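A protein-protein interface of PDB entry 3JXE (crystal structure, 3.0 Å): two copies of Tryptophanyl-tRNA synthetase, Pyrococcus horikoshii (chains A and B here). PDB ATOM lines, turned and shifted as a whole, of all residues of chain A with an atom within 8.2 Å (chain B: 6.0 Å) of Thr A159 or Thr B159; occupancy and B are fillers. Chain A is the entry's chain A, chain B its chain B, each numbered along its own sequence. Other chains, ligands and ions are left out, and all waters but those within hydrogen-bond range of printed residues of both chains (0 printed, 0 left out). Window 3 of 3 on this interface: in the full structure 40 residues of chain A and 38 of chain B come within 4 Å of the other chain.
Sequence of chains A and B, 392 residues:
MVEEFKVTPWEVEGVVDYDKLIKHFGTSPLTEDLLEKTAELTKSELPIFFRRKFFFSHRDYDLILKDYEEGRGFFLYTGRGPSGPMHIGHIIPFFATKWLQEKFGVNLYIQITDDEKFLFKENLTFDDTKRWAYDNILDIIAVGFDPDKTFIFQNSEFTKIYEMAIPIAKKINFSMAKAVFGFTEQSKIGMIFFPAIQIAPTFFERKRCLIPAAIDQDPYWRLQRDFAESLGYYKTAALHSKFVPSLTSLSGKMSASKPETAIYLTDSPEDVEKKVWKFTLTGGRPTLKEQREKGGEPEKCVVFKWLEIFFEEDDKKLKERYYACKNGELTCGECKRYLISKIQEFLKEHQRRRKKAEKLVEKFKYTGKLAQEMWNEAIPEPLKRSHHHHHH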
ATOM      1  N   ASP A 115     -13.347 -35.018 -12.666  1.00  0.00           N
ATOM      2  CA  ASP A 115     -14.410 -34.063 -12.961  1.00  0.00           C
ATOM      3  C   ASP A 115     -15.786 -34.710 -12.814  1.00  0.00           C
ATOM      4  O   ASP A 115     -16.688 -34.120 -12.220  1.00  0.00           O
ATOM      5  CB  ASP A 115     -14.234 -33.439 -14.354  1.00  0.00           C
ATOM      6  CG  ASP A 115     -14.121 -34.476 -15.468  1.00  0.00           C
ATOM      7  OD1 ASP A 115     -13.841 -35.662 -15.189  1.00  0.00           O
ATOM      8  OD2 ASP A 115     -14.301 -34.092 -16.641  1.00  0.00           O
ATOM      9  N   PHE A 126     -14.476 -31.004  -5.159  1.00  0.00           N
ATOM     10  CA  PHE A 126     -13.540 -31.129  -6.279  1.00  0.00           C
ATOM     11  C   PHE A 126     -12.130 -31.395  -5.768  1.00  0.00           C
ATOM     12  O   PHE A 126     -11.336 -32.069  -6.424  1.00  0.00           O
ATOM     13  CB  PHE A 126     -13.572 -29.866  -7.152  1.00  0.00           C
ATOM     14  CG  PHE A 126     -13.057 -30.070  -8.560  1.00  0.00           C
ATOM     15  CD1 PHE A 126     -12.622 -28.983  -9.311  1.00  0.00           C
ATOM     16  CD2 PHE A 126     -13.008 -31.341  -9.135  1.00  0.00           C
ATOM     17  CE1 PHE A 126     -12.152 -29.156 -10.614  1.00  0.00           C
ATOM     18  CE2 PHE A 126     -12.534 -31.524 -10.431  1.00  0.00           C
ATOM     19  CZ  PHE A 126     -12.108 -30.428 -11.172  1.00  0.00           C
ATOM     20  N   PHE A 151      -0.398 -43.484 -21.191  1.00  0.00           N
ATOM     21  CA  PHE A 151      -0.665 -42.131 -20.720  1.00  0.00           C
ATOM     22  C   PHE A 151      -1.818 -42.124 -19.721  1.00  0.00           C
ATOM     23  O   PHE A 151      -2.950 -42.476 -20.058  1.00  0.00           O
ATOM     24  CB  PHE A 151      -0.956 -41.196 -21.901  1.00  0.00           C
ATOM     25  CG  PHE A 151      -1.229 -39.763 -21.507  1.00  0.00           C
ATOM     26  CD1 PHE A 151      -0.411 -39.101 -20.594  1.00  0.00           C
ATOM     27  CD2 PHE A 151      -2.289 -39.069 -22.076  1.00  0.00           C
ATOM     28  CE1 PHE A 151      -0.657 -37.777 -20.241  1.00  0.00           C
ATOM     29  CE2 PHE A 151      -2.542 -37.742 -21.731  1.00  0.00           C
ATOM     30  CZ  PHE A 151      -1.723 -37.097 -20.813  1.00  0.00           C
ATOM     31  N   PHE A 153      -3.986 -39.699 -17.262  1.00  0.00           N
ATOM     32  CA  PHE A 153      -4.327 -38.285 -17.108  1.00  0.00           C
ATOM     33  C   PHE A 153      -5.619 -38.045 -16.332  1.00  0.00           C
ATOM     34  O   PHE A 153      -6.529 -38.877 -16.342  1.00  0.00           O
ATOM     35  CB  PHE A 153      -4.404 -37.601 -18.480  1.00  0.00           C
ATOM     36  CG  PHE A 153      -5.564 -38.056 -19.329  1.00  0.00           C
ATOM     37  CD1 PHE A 153      -5.480 -39.225 -20.082  1.00  0.00           C
ATOM     38  CD2 PHE A 153      -6.739 -37.310 -19.383  1.00  0.00           C
ATOM     39  CE1 PHE A 153      -6.549 -39.647 -20.865  1.00  0.00           C
ATOM     40  CE2 PHE A 153      -7.813 -37.726 -20.163  1.00  0.00           C
ATOM     41  CZ  PHE A 153      -7.716 -38.896 -20.907  1.00  0.00           C
ATOM     42  N   GLN A 154      -5.681 -36.896 -15.664  1.00  0.00           N
ATOM     43  CA  GLN A 154      -6.901 -36.428 -15.021  1.00  0.00           C
ATOM     44  C   GLN A 154      -7.527 -35.343 -15.885  1.00  0.00           C
ATOM     45  O   GLN A 154      -6.823 -34.470 -16.397  1.00  0.00           O
ATOM     46  CB  GLN A 154      -6.598 -35.860 -13.636  1.00  0.00           C
ATOM     47  CG  GLN A 154      -6.111 -36.880 -12.619  1.00  0.00           C
ATOM     48  CD  GLN A 154      -5.596 -36.229 -11.347  1.00  0.00           C
ATOM     49  OE1 GLN A 154      -4.486 -36.514 -10.900  1.00  0.00           O
ATOM     50  NE2 GLN A 154      -6.399 -35.347 -10.759  1.00  0.00           N
ATOM     51  N   ASN A 155      -8.848 -35.397 -16.037  1.00  0.00           N
ATOM     52  CA  ASN A 155      -9.578 -34.439 -16.868  1.00  0.00           C
ATOM     53  C   ASN A 155      -9.413 -32.988 -16.422  1.00  0.00           C
ATOM     54  O   ASN A 155      -9.463 -32.076 -17.244  1.00  0.00           O
ATOM     55  CB  ASN A 155     -11.063 -34.796 -16.927  1.00  0.00           C
ATOM     56  CG  ASN A 155     -11.331 -36.081 -17.689  1.00  0.00           C
ATOM     57  OD1 ASN A 155     -10.647 -36.398 -18.663  1.00  0.00           O
ATOM     58  ND2 ASN A 155     -12.342 -36.824 -17.252  1.00  0.00           N
ATOM     59  N   SER A 156      -9.214 -32.789 -15.122  1.00  0.00           N
ATOM     60  CA  SER A 156      -9.015 -31.456 -14.553  1.00  0.00           C
ATOM     61  C   SER A 156      -7.621 -30.898 -14.848  1.00  0.00           C
ATOM     62  O   SER A 156      -7.408 -29.685 -14.802  1.00  0.00           O
ATOM     63  CB  SER A 156      -9.262 -31.482 -13.042  1.00  0.00           C
ATOM     64  OG  SER A 156      -8.317 -32.302 -12.377  1.00  0.00           O
ATOM     65  N   GLU A 157      -6.679 -31.790 -15.146  1.00  0.00           N
ATOM     66  CA  GLU A 157      -5.288 -31.409 -15.378  1.00  0.00           C
ATOM     67  C   GLU A 157      -4.965 -31.364 -16.870  1.00  0.00           C
ATOM     68  O   GLU A 157      -4.577 -30.320 -17.394  1.00  0.00           O
ATOM     69  CB  GLU A 157      -4.355 -32.378 -14.653  1.00  0.00           C
ATOM     70  CG  GLU A 157      -2.934 -31.878 -14.479  1.00  0.00           C
ATOM     71  CD  GLU A 157      -2.062 -32.879 -13.754  1.00  0.00           C
ATOM     72  OE1 GLU A 157      -2.213 -34.094 -14.001  1.00  0.00           O
ATOM     73  OE2 GLU A 157      -1.223 -32.453 -12.935  1.00  0.00           O
ATOM     74  N   PHE A 158      -5.121 -32.503 -17.540  1.00  0.00           N
ATOM     75  CA  PHE A 158      -4.979 -32.581 -18.990  1.00  0.00           C
ATOM     76  C   PHE A 158      -6.297 -32.140 -19.621  1.00  0.00           C
ATOM     77  O   PHE A 158      -7.042 -32.949 -20.179  1.00  0.00           O
ATOM     78  CB  PHE A 158      -4.594 -34.004 -19.413  1.00  0.00           C
ATOM     79  CG  PHE A 158      -4.312 -34.155 -20.886  1.00  0.00           C
ATOM     80  CD1 PHE A 158      -3.193 -33.556 -21.464  1.00  0.00           C
ATOM     81  CD2 PHE A 158      -5.158 -34.915 -21.694  1.00  0.00           C
ATOM     82  CE1 PHE A 158      -2.929 -33.702 -22.827  1.00  0.00           C
ATOM     83  CE2 PHE A 158      -4.901 -35.066 -23.059  1.00  0.00           C
ATOM     84  CZ  PHE A 158      -3.783 -34.459 -23.625  1.00  0.00           C
ATOM     85  N   THR A 159      -6.575 -30.841 -19.524  1.00  0.00           N
ATOM     86  CA  THR A 159      -7.856 -30.280 -19.948  1.00  0.00           C
ATOM     87  C   THR A 159      -8.054 -30.243 -21.467  1.00  0.00           C
ATOM     88  O   THR A 159      -9.058 -29.721 -21.954  1.00  0.00           O
ATOM     89  CB  THR A 159      -8.081 -28.866 -19.367  1.00  0.00           C
ATOM     90  OG1 THR A 159      -6.929 -28.051 -19.607  1.00  0.00           O
ATOM     91  CG2 THR A 159      -8.357 -28.933 -17.873  1.00  0.00           C
ATOM     92  N   LYS A 160      -7.110 -30.815 -22.212  1.00  0.00           N
ATOM     93  CA  LYS A 160      -7.239 -30.905 -23.661  1.00  0.00           C
ATOM     94  C   LYS A 160      -8.441 -31.762 -24.075  1.00  0.00           C
ATOM     95  O   LYS A 160      -8.949 -31.619 -25.191  1.00  0.00           O
ATOM     96  CB  LYS A 160      -5.956 -31.442 -24.300  1.00  0.00           C
ATOM     97  CG  LYS A 160      -5.807 -31.054 -25.765  1.00  0.00           C
ATOM     98  CD  LYS A 160      -5.144 -32.166 -26.578  1.00  0.00           C
ATOM     99  CE  LYS A 160      -5.448 -32.017 -28.071  1.00  0.00           C
ATOM    100  NZ  LYS A 160      -4.872 -30.754 -28.653  1.00  0.00           N
ATOM    101  N   ILE A 161      -8.899 -32.640 -23.180  1.00  0.00           N
ATOM    102  CA  ILE A 161     -10.094 -33.453 -23.445  1.00  0.00           C
ATOM    103  C   ILE A 161     -11.326 -32.604 -23.726  1.00  0.00           C
ATOM    104  O   ILE A 161     -12.220 -33.039 -24.447  1.00  0.00           O
ATOM    105  CB  ILE A 161     -10.421 -34.480 -22.322  1.00  0.00           C
ATOM    106  CG1 ILE A 161      -9.873 -34.028 -20.965  1.00  0.00           C
ATOM    107  CG2 ILE A 161      -9.897 -35.862 -22.691  1.00  0.00           C
ATOM    108  CD1 ILE A 161     -10.706 -32.981 -20.263  1.00  0.00           C
ATOM    109  N   TYR A 162     -11.373 -31.400 -23.157  1.00  0.00           N
ATOM    110  CA  TYR A 162     -12.468 -30.477 -23.435  1.00  0.00           C
ATOM    111  C   TYR A 162     -12.496 -30.111 -24.917  1.00  0.00           C
ATOM    112  O   TYR A 162     -13.552 -30.149 -25.550  1.00  0.00           O
ATOM    113  CB  TYR A 162     -12.381 -29.218 -22.570  1.00  0.00           C
ATOM    114  CG  TYR A 162     -13.445 -28.193 -22.905  1.00  0.00           C
ATOM    115  CD1 TYR A 162     -14.794 -28.452 -22.656  1.00  0.00           C
ATOM    116  CD2 TYR A 162     -13.107 -26.968 -23.481  1.00  0.00           C
ATOM    117  CE1 TYR A 162     -15.774 -27.523 -22.965  1.00  0.00           C
ATOM    118  CE2 TYR A 162     -14.083 -26.027 -23.792  1.00  0.00           C
ATOM    119  CZ  TYR A 162     -15.414 -26.314 -23.532  1.00  0.00           C
ATOM    120  OH  TYR A 162     -16.390 -25.394 -23.836  1.00  0.00           O
ATOM    121  N   GLU A 163     -11.329 -29.771 -25.459  1.00  0.00           N
ATOM    122  CA  GLU A 163     -11.181 -29.462 -26.876  1.00  0.00           C
ATOM    123  C   GLU A 163     -11.396 -30.712 -27.733  1.00  0.00           C
ATOM    124  O   GLU A 163     -11.875 -30.623 -28.861  1.00  0.00           O
ATOM    125  CB  GLU A 163      -9.804 -28.849 -27.134  1.00  0.00           C
ATOM    126  CG  GLU A 163      -9.649 -28.173 -28.491  1.00  0.00           C
ATOM    127  CD  GLU A 163      -9.038 -29.075 -29.555  1.00  0.00           C
ATOM    128  OE1 GLU A 163      -8.755 -30.262 -29.269  1.00  0.00           O
ATOM    129  OE2 GLU A 163      -8.835 -28.586 -30.688  1.00  0.00           O
ATOM    130  N   MET A 164     -11.044 -31.870 -27.183  1.00  0.00           N
ATOM    131  CA  MET A 164     -11.256 -33.151 -27.851  1.00  0.00           C
ATOM    132  C   MET A 164     -12.723 -33.588 -27.825  1.00  0.00           C
ATOM    133  O   MET A 164     -13.139 -34.423 -28.632  1.00  0.00           O
ATOM    134  CB  MET A 164     -10.385 -34.236 -27.213  1.00  0.00           C
ATOM    135  CG  MET A 164      -8.893 -34.094 -27.484  1.00  0.00           C
ATOM    136  SD  MET A 164      -7.878 -35.228 -26.512  1.00  0.00           S
ATOM    137  CE  MET A 164      -8.328 -36.816 -27.211  1.00  0.00           C
ATOM    138  N   ALA A 165     -13.497 -33.019 -26.902  1.00  0.00           N
ATOM    139  CA  ALA A 165     -14.898 -33.404 -26.696  1.00  0.00           C
ATOM    140  C   ALA A 165     -15.895 -32.531 -27.455  1.00  0.00           C
ATOM    141  O   ALA A 165     -17.024 -32.949 -27.702  1.00  0.00           O
ATOM    142  CB  ALA A 165     -15.230 -33.399 -25.214  1.00  0.00           C
ATOM    143  N   ILE A 166     -15.475 -31.323 -27.816  1.00  0.00           N
ATOM    144  CA  ILE A 166     -16.359 -30.351 -28.463  1.00  0.00           C
ATOM    145  C   ILE A 166     -17.012 -30.846 -29.774  1.00  0.00           C
ATOM    146  O   ILE A 166     -18.217 -30.648 -29.960  1.00  0.00           O
ATOM    147  CB  ILE A 166     -15.661 -28.974 -28.620  1.00  0.00           C
ATOM    148  CG1 ILE A 166     -15.622 -28.259 -27.270  1.00  0.00           C
ATOM    149  CG2 ILE A 166     -16.382 -28.096 -29.632  1.00  0.00           C
ATOM    150  CD1 ILE A 166     -14.465 -27.297 -27.121  1.00  0.00           C
ATOM    151  N   ILE A 197     -16.923 -35.912 -22.697  1.00  0.00           N
ATOM    152  CA  ILE A 197     -15.594 -36.063 -22.100  1.00  0.00           C
ATOM    153  C   ILE A 197     -15.126 -37.525 -22.066  1.00  0.00           C
ATOM    154  O   ILE A 197     -13.965 -37.807 -22.359  1.00  0.00           O
ATOM    155  CB  ILE A 197     -15.541 -35.422 -20.678  1.00  0.00           C
ATOM    156  CG1 ILE A 197     -15.785 -33.906 -20.747  1.00  0.00           C
ATOM    157  CG2 ILE A 197     -14.235 -35.754 -19.946  1.00  0.00           C
ATOM    158  CD1 ILE A 197     -14.662 -33.089 -21.394  1.00  0.00           C
ATOM    159  N   TRP A 375       1.387 -34.208 -23.955  1.00  0.00           N
ATOM    160  CA  TRP A 375       1.538 -32.917 -23.281  1.00  0.00           C
ATOM    161  C   TRP A 375       2.124 -31.828 -24.177  1.00  0.00           C
ATOM    162  O   TRP A 375       1.964 -30.636 -23.898  1.00  0.00           O
ATOM    163  CB  TRP A 375       2.339 -33.057 -21.984  1.00  0.00           C
ATOM    164  CG  TRP A 375       1.485 -33.420 -20.807  1.00  0.00           C
ATOM    165  CD1 TRP A 375       1.487 -34.601 -20.126  1.00  0.00           C
ATOM    166  CD2 TRP A 375       0.489 -32.598 -20.181  1.00  0.00           C
ATOM    167  NE1 TRP A 375       0.562 -34.567 -19.110  1.00  0.00           N
ATOM    168  CE2 TRP A 375      -0.066 -33.350 -19.122  1.00  0.00           C
ATOM    169  CE3 TRP A 375       0.013 -31.299 -20.412  1.00  0.00           C
ATOM    170  CZ2 TRP A 375      -1.073 -32.845 -18.291  1.00  0.00           C
ATOM    171  CZ3 TRP A 375      -0.989 -30.799 -19.584  1.00  0.00           C
ATOM    172  CH2 TRP A 375      -1.518 -31.572 -18.537  1.00  0.00           C
ATOM    173  N   GLU A 377       0.937 -30.725 -26.527  1.00  0.00           N
ATOM    174  CA  GLU A 377      -0.241 -30.055 -27.096  1.00  0.00           C
ATOM    175  C   GLU A 377      -0.434 -28.667 -26.453  1.00  0.00           C
ATOM    176  O   GLU A 377      -1.417 -27.965 -26.735  1.00  0.00           O
ATOM    177  CB  GLU A 377      -1.485 -30.935 -26.912  1.00  0.00           C
ATOM    178  CG  GLU A 377      -1.697 -31.992 -28.006  1.00  0.00           C
ATOM    179  CD  GLU A 377      -0.532 -32.082 -28.997  1.00  0.00           C
ATOM    180  OE1 GLU A 377      -0.569 -31.358 -30.023  1.00  0.00           O
ATOM    181  OE2 GLU A 377       0.410 -32.879 -28.756  1.00  0.00           O
ATOM    182  N   ALA A 378       0.517 -28.287 -25.580  1.00  0.00           N
ATOM    183  CA  ALA A 378       0.621 -26.912 -25.080  1.00  0.00           C
ATOM    184  C   ALA A 378       1.264 -26.063 -26.189  1.00  0.00           C
ATOM    185  O   ALA A 378       2.303 -26.439 -26.783  1.00  0.00           O
ATOM    186  CB  ALA A 378       1.437 -26.816 -23.840  1.00  0.00           C
ATOM    187  N   GLN B 154      -8.122 -18.410 -25.971  1.00  0.00           N
ATOM    188  CA  GLN B 154      -9.095 -19.106 -26.789  1.00  0.00           C
ATOM    189  C   GLN B 154      -9.514 -20.356 -26.024  1.00  0.00           C
ATOM    190  O   GLN B 154      -8.661 -21.141 -25.603  1.00  0.00           O
ATOM    191  CB  GLN B 154      -8.425 -19.502 -28.097  1.00  0.00           C
ATOM    192  CG  GLN B 154      -9.166 -19.113 -29.349  1.00  0.00           C
ATOM    193  CD  GLN B 154      -8.308 -19.303 -30.583  1.00  0.00           C
ATOM    194  OE1 GLN B 154      -7.316 -18.600 -30.777  1.00  0.00           O
ATOM    195  NE2 GLN B 154      -8.685 -20.258 -31.426  1.00  0.00           N
ATOM    196  N   ASN B 155     -10.818 -20.543 -25.838  1.00  0.00           N
ATOM    197  CA  ASN B 155     -11.335 -21.655 -25.029  1.00  0.00           C
ATOM    198  C   ASN B 155     -10.831 -23.038 -25.444  1.00  0.00           C
ATOM    199  O   ASN B 155     -10.666 -23.918 -24.599  1.00  0.00           O
ATOM    200  CB  ASN B 155     -12.864 -21.649 -25.003  1.00  0.00           C
ATOM    201  CG  ASN B 155     -13.437 -20.514 -24.174  1.00  0.00           C
ATOM    202  OD1 ASN B 155     -12.798 -20.013 -23.246  1.00  0.00           O
ATOM    203  ND2 ASN B 155     -14.660 -20.107 -24.502  1.00  0.00           N
ATOM    204  N   SER B 156     -10.590 -23.218 -26.740  1.00  0.00           N
ATOM    205  CA  SER B 156     -10.093 -24.484 -27.279  1.00  0.00           C
ATOM    206  C   SER B 156      -8.598 -24.682 -27.020  1.00  0.00           C
ATOM    207  O   SER B 156      -8.084 -25.798 -27.102  1.00  0.00           O
ATOM    208  CB  SER B 156     -10.376 -24.566 -28.782  1.00  0.00           C
ATOM    209  OG  SER B 156      -9.628 -23.601 -29.501  1.00  0.00           O
ATOM    210  N   GLU B 157      -7.909 -23.590 -26.705  1.00  0.00           N
ATOM    211  CA  GLU B 157      -6.460 -23.594 -26.558  1.00  0.00           C
ATOM    212  C   GLU B 157      -6.059 -23.508 -25.089  1.00  0.00           C
ATOM    213  O   GLU B 157      -5.336 -24.369 -24.585  1.00  0.00           O
ATOM    214  CB  GLU B 157      -5.877 -22.425 -27.345  1.00  0.00           C
ATOM    215  CG  GLU B 157      -4.378 -22.435 -27.506  1.00  0.00           C
ATOM    216  CD  GLU B 157      -3.880 -21.120 -28.050  1.00  0.00           C
ATOM    217  OE1 GLU B 157      -4.313 -20.064 -27.538  1.00  0.00           O
ATOM    218  OE2 GLU B 157      -3.065 -21.140 -28.995  1.00  0.00           O
ATOM    219  N   PHE B 158      -6.524 -22.461 -24.414  1.00  0.00           N
ATOM    220  CA  PHE B 158      -6.373 -22.334 -22.971  1.00  0.00           C
ATOM    221  C   PHE B 158      -7.519 -23.103 -22.321  1.00  0.00           C
ATOM    222  O   PHE B 158      -8.435 -22.515 -21.741  1.00  0.00           O
ATOM    223  CB  PHE B 158      -6.376 -20.856 -22.559  1.00  0.00           C
ATOM    224  CG  PHE B 158      -6.143 -20.622 -21.089  1.00  0.00           C
ATOM    225  CD1 PHE B 158      -7.169 -20.133 -20.279  1.00  0.00           C
ATOM    226  CD2 PHE B 158      -4.900 -20.879 -20.512  1.00  0.00           C
ATOM    227  CE1 PHE B 158      -6.962 -19.910 -18.916  1.00  0.00           C
ATOM    228  CE2 PHE B 158      -4.682 -20.659 -19.151  1.00  0.00           C
ATOM    229  CZ  PHE B 158      -5.714 -20.170 -18.353  1.00  0.00           C
ATOM    230  N   THR B 159      -7.454 -24.430 -22.431  1.00  0.00           N
ATOM    231  CA  THR B 159      -8.527 -25.312 -21.975  1.00  0.00           C
ATOM    232  C   THR B 159      -8.661 -25.365 -20.452  1.00  0.00           C
ATOM    233  O   THR B 159      -9.475 -26.119 -19.916  1.00  0.00           O
ATOM    234  CB  THR B 159      -8.372 -26.739 -22.536  1.00  0.00           C
ATOM    235  OG1 THR B 159      -7.030 -27.199 -22.342  1.00  0.00           O
ATOM    236  CG2 THR B 159      -8.716 -26.776 -24.016  1.00  0.00           C
ATOM    237  N   LYS B 160      -7.876 -24.542 -19.766  1.00  0.00           N
ATOM    238  CA  LYS B 160      -7.923 -24.441 -18.316  1.00  0.00           C
ATOM    239  C   LYS B 160      -9.303 -23.997 -17.812  1.00  0.00           C
ATOM    240  O   LYS B 160      -9.696 -24.356 -16.698  1.00  0.00           O
ATOM    241  CB  LYS B 160      -6.828 -23.487 -17.821  1.00  0.00           C
ATOM    242  CG  LYS B 160      -6.250 -23.816 -16.449  1.00  0.00           C
ATOM    243  CD  LYS B 160      -6.964 -23.058 -15.330  1.00  0.00           C
ATOM    244  CE  LYS B 160      -6.219 -23.169 -14.004  1.00  0.00           C
ATOM    245  NZ  LYS B 160      -6.139 -24.576 -13.508  1.00  0.00           N
ATOM    246  N   ILE B 161     -10.044 -23.239 -18.627  1.00  0.00           N
ATOM    247  CA  ILE B 161     -11.390 -22.791 -18.230  1.00  0.00           C
ATOM    248  C   ILE B 161     -12.358 -23.944 -18.008  1.00  0.00           C
ATOM    249  O   ILE B 161     -13.354 -23.782 -17.305  1.00  0.00           O
ATOM    250  CB  ILE B 161     -12.045 -21.718 -19.178  1.00  0.00           C
ATOM    251  CG1 ILE B 161     -12.456 -22.294 -20.552  1.00  0.00           C
ATOM    252  CG2 ILE B 161     -11.204 -20.447 -19.249  1.00  0.00           C
ATOM    253  CD1 ILE B 161     -11.373 -22.995 -21.352  1.00  0.00           C
ATOM    254  N   TYR B 162     -12.073 -25.102 -18.601  1.00  0.00           N
ATOM    255  CA  TYR B 162     -12.872 -26.287 -18.323  1.00  0.00           C
ATOM    256  C   TYR B 162     -12.791 -26.644 -16.837  1.00  0.00           C
ATOM    257  O   TYR B 162     -13.815 -26.868 -16.195  1.00  0.00           O
ATOM    258  CB  TYR B 162     -12.460 -27.476 -19.192  1.00  0.00           C
ATOM    259  CG  TYR B 162     -13.240 -28.729 -18.867  1.00  0.00           C
ATOM    260  CD1 TYR B 162     -12.619 -29.825 -18.266  1.00  0.00           C
ATOM    261  CD2 TYR B 162     -14.608 -28.807 -19.128  1.00  0.00           C
ATOM    262  CE1 TYR B 162     -13.338 -30.973 -17.954  1.00  0.00           C
ATOM    263  CE2 TYR B 162     -15.334 -29.947 -18.822  1.00  0.00           C
ATOM    264  CZ  TYR B 162     -14.694 -31.025 -18.236  1.00  0.00           C
ATOM    265  OH  TYR B 162     -15.416 -32.153 -17.931  1.00  0.00           O
ATOM    266  N   GLU B 163     -11.572 -26.675 -16.300  1.00  0.00           N
ATOM    267  CA  GLU B 163     -11.351 -26.907 -14.875  1.00  0.00           C
ATOM    268  C   GLU B 163     -11.888 -25.739 -14.041  1.00  0.00           C
ATOM    269  O   GLU B 163     -12.307 -25.926 -12.901  1.00  0.00           O
ATOM    270  CB  GLU B 163      -9.863 -27.144 -14.605  1.00  0.00           C
ATOM    271  CG  GLU B 163      -9.531 -27.730 -13.232  1.00  0.00           C
ATOM    272  CD  GLU B 163      -9.328 -26.670 -12.158  1.00  0.00           C
ATOM    273  OE1 GLU B 163      -8.839 -25.563 -12.488  1.00  0.00           O
ATOM    274  OE2 GLU B 163      -9.653 -26.944 -10.980  1.00  0.00           O
ATOM    275  N   TRP B 375      -0.518 -19.060 -18.075  1.00  0.00           N
ATOM    276  CA  TRP B 375      -0.056 -20.262 -18.767  1.00  0.00           C
ATOM    277  C   TRP B 375       0.794 -21.176 -17.887  1.00  0.00           C
ATOM    278  O   TRP B 375       0.967 -22.358 -18.197  1.00  0.00           O
ATOM    279  CB  TRP B 375       0.658 -19.919 -20.076  1.00  0.00           C
ATOM    280  CG  TRP B 375      -0.289 -19.801 -21.228  1.00  0.00           C
ATOM    281  CD1 TRP B 375      -0.624 -18.663 -21.898  1.00  0.00           C
ATOM    282  CD2 TRP B 375      -1.045 -20.860 -21.829  1.00  0.00           C
ATOM    283  NE1 TRP B 375      -1.533 -18.947 -22.888  1.00  0.00           N
ATOM    284  CE2 TRP B 375      -1.810 -20.288 -22.868  1.00  0.00           C
ATOM    285  CE3 TRP B 375      -1.148 -22.238 -21.594  1.00  0.00           C
ATOM    286  CZ2 TRP B 375      -2.668 -21.044 -23.671  1.00  0.00           C
ATOM    287  CZ3 TRP B 375      -2.000 -22.989 -22.396  1.00  0.00           C
ATOM    288  CH2 TRP B 375      -2.748 -22.388 -23.422  1.00  0.00           C
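The side-chain amino group (NZ) of Lys B160 lies within salt-bridge range of the side-chain carboxylate (OE1) of Glu B163. OE1 of Glu A163 is in salt-bridge range of NZ of Lys A160 (3.96 Å). ND2 of Asn A155 lies within hydrogen-bond range of OD1 of Asp A115 (2.8 Å).
Printed residues of chain B that touch a printed residue of chain A: Ser B156, Thr B159, Lys B160, Tyr B162 and Glu B163. Along chain B the printed residues that touch a printed residue of chain A span positions 156 to 163. Of the 21 printed residues of chain A, 8 touch a printed residue of chain B. Hydrophobic or aromatic side chains of chain A that line the printed part of chain B: Phe A126, Tyr A162 and Ile A197. Among the printed residues, 10 pairs touch across the chains. Among the printed residues, no Asp or Glu carboxylate lies within 4 Å of a Lys or Arg side-chain nitrogen of the other chain.
The side-chain hydroxyl of Thr A159 is in hydrogen-bond range of the side-chain hydroxyl of Thr B159, at 2.9 Å. OD2 of Asp A115 sits at hydrogen-bond distance from OH of Tyr B162 (2.6 Å).
Ser A156 touches Glu B163, and with the chains exchanged Glu A163 touches Ser B156. Thr B159 touches its own counterpart, Thr A159. Thr A159 touches Lys B160, and with the chains exchanged Lys A160 touches Thr B159. Glu A163 touches Thr B159, but with the chains exchanged Thr A159 does not touch Glu B163 (4.02 Å). 11 positions are printed for both chains. Of the 10 pairs that touch across the chains among the printed residues, 6 have their exchanged pair printed and touching as well.
Among the printed residues, pairs that only touch across the chains: Glu A163 with Ser B156 (3.2 Å), Ser A156 with Glu B163 (3.3 Å), Ile A197 with Tyr B162 (3.3 Å), Phe A126 with Glu B163 (3.4 Å), Tyr A162 with Tyr B162 (3.6 Å), Lys A160 with Thr B159 (3.6 Å), Thr A159 with Lys B160 (3.6 Å) and Glu A163 with Thr B159 (3.9 Å).
Of the printed residues of chain B, Phe A126 touches Glu B163 (3.4 Å). Printed residues of chain B within 4 Å of Thr A159: Thr B159 and Lys B160. Glu B157 touches none of the printed residues of chain A. Thr B159 touches just these residues of chain A: Thr A159 (2.9 Å), Lys A160 (3.6 Å) and Glu A163 (3.9 Å). Printed residues of chain A within 4 Å of Lys B160: Thr A159. Of the printed residues of chain A, Glu B163 touches Phe A126 and Ser A156.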
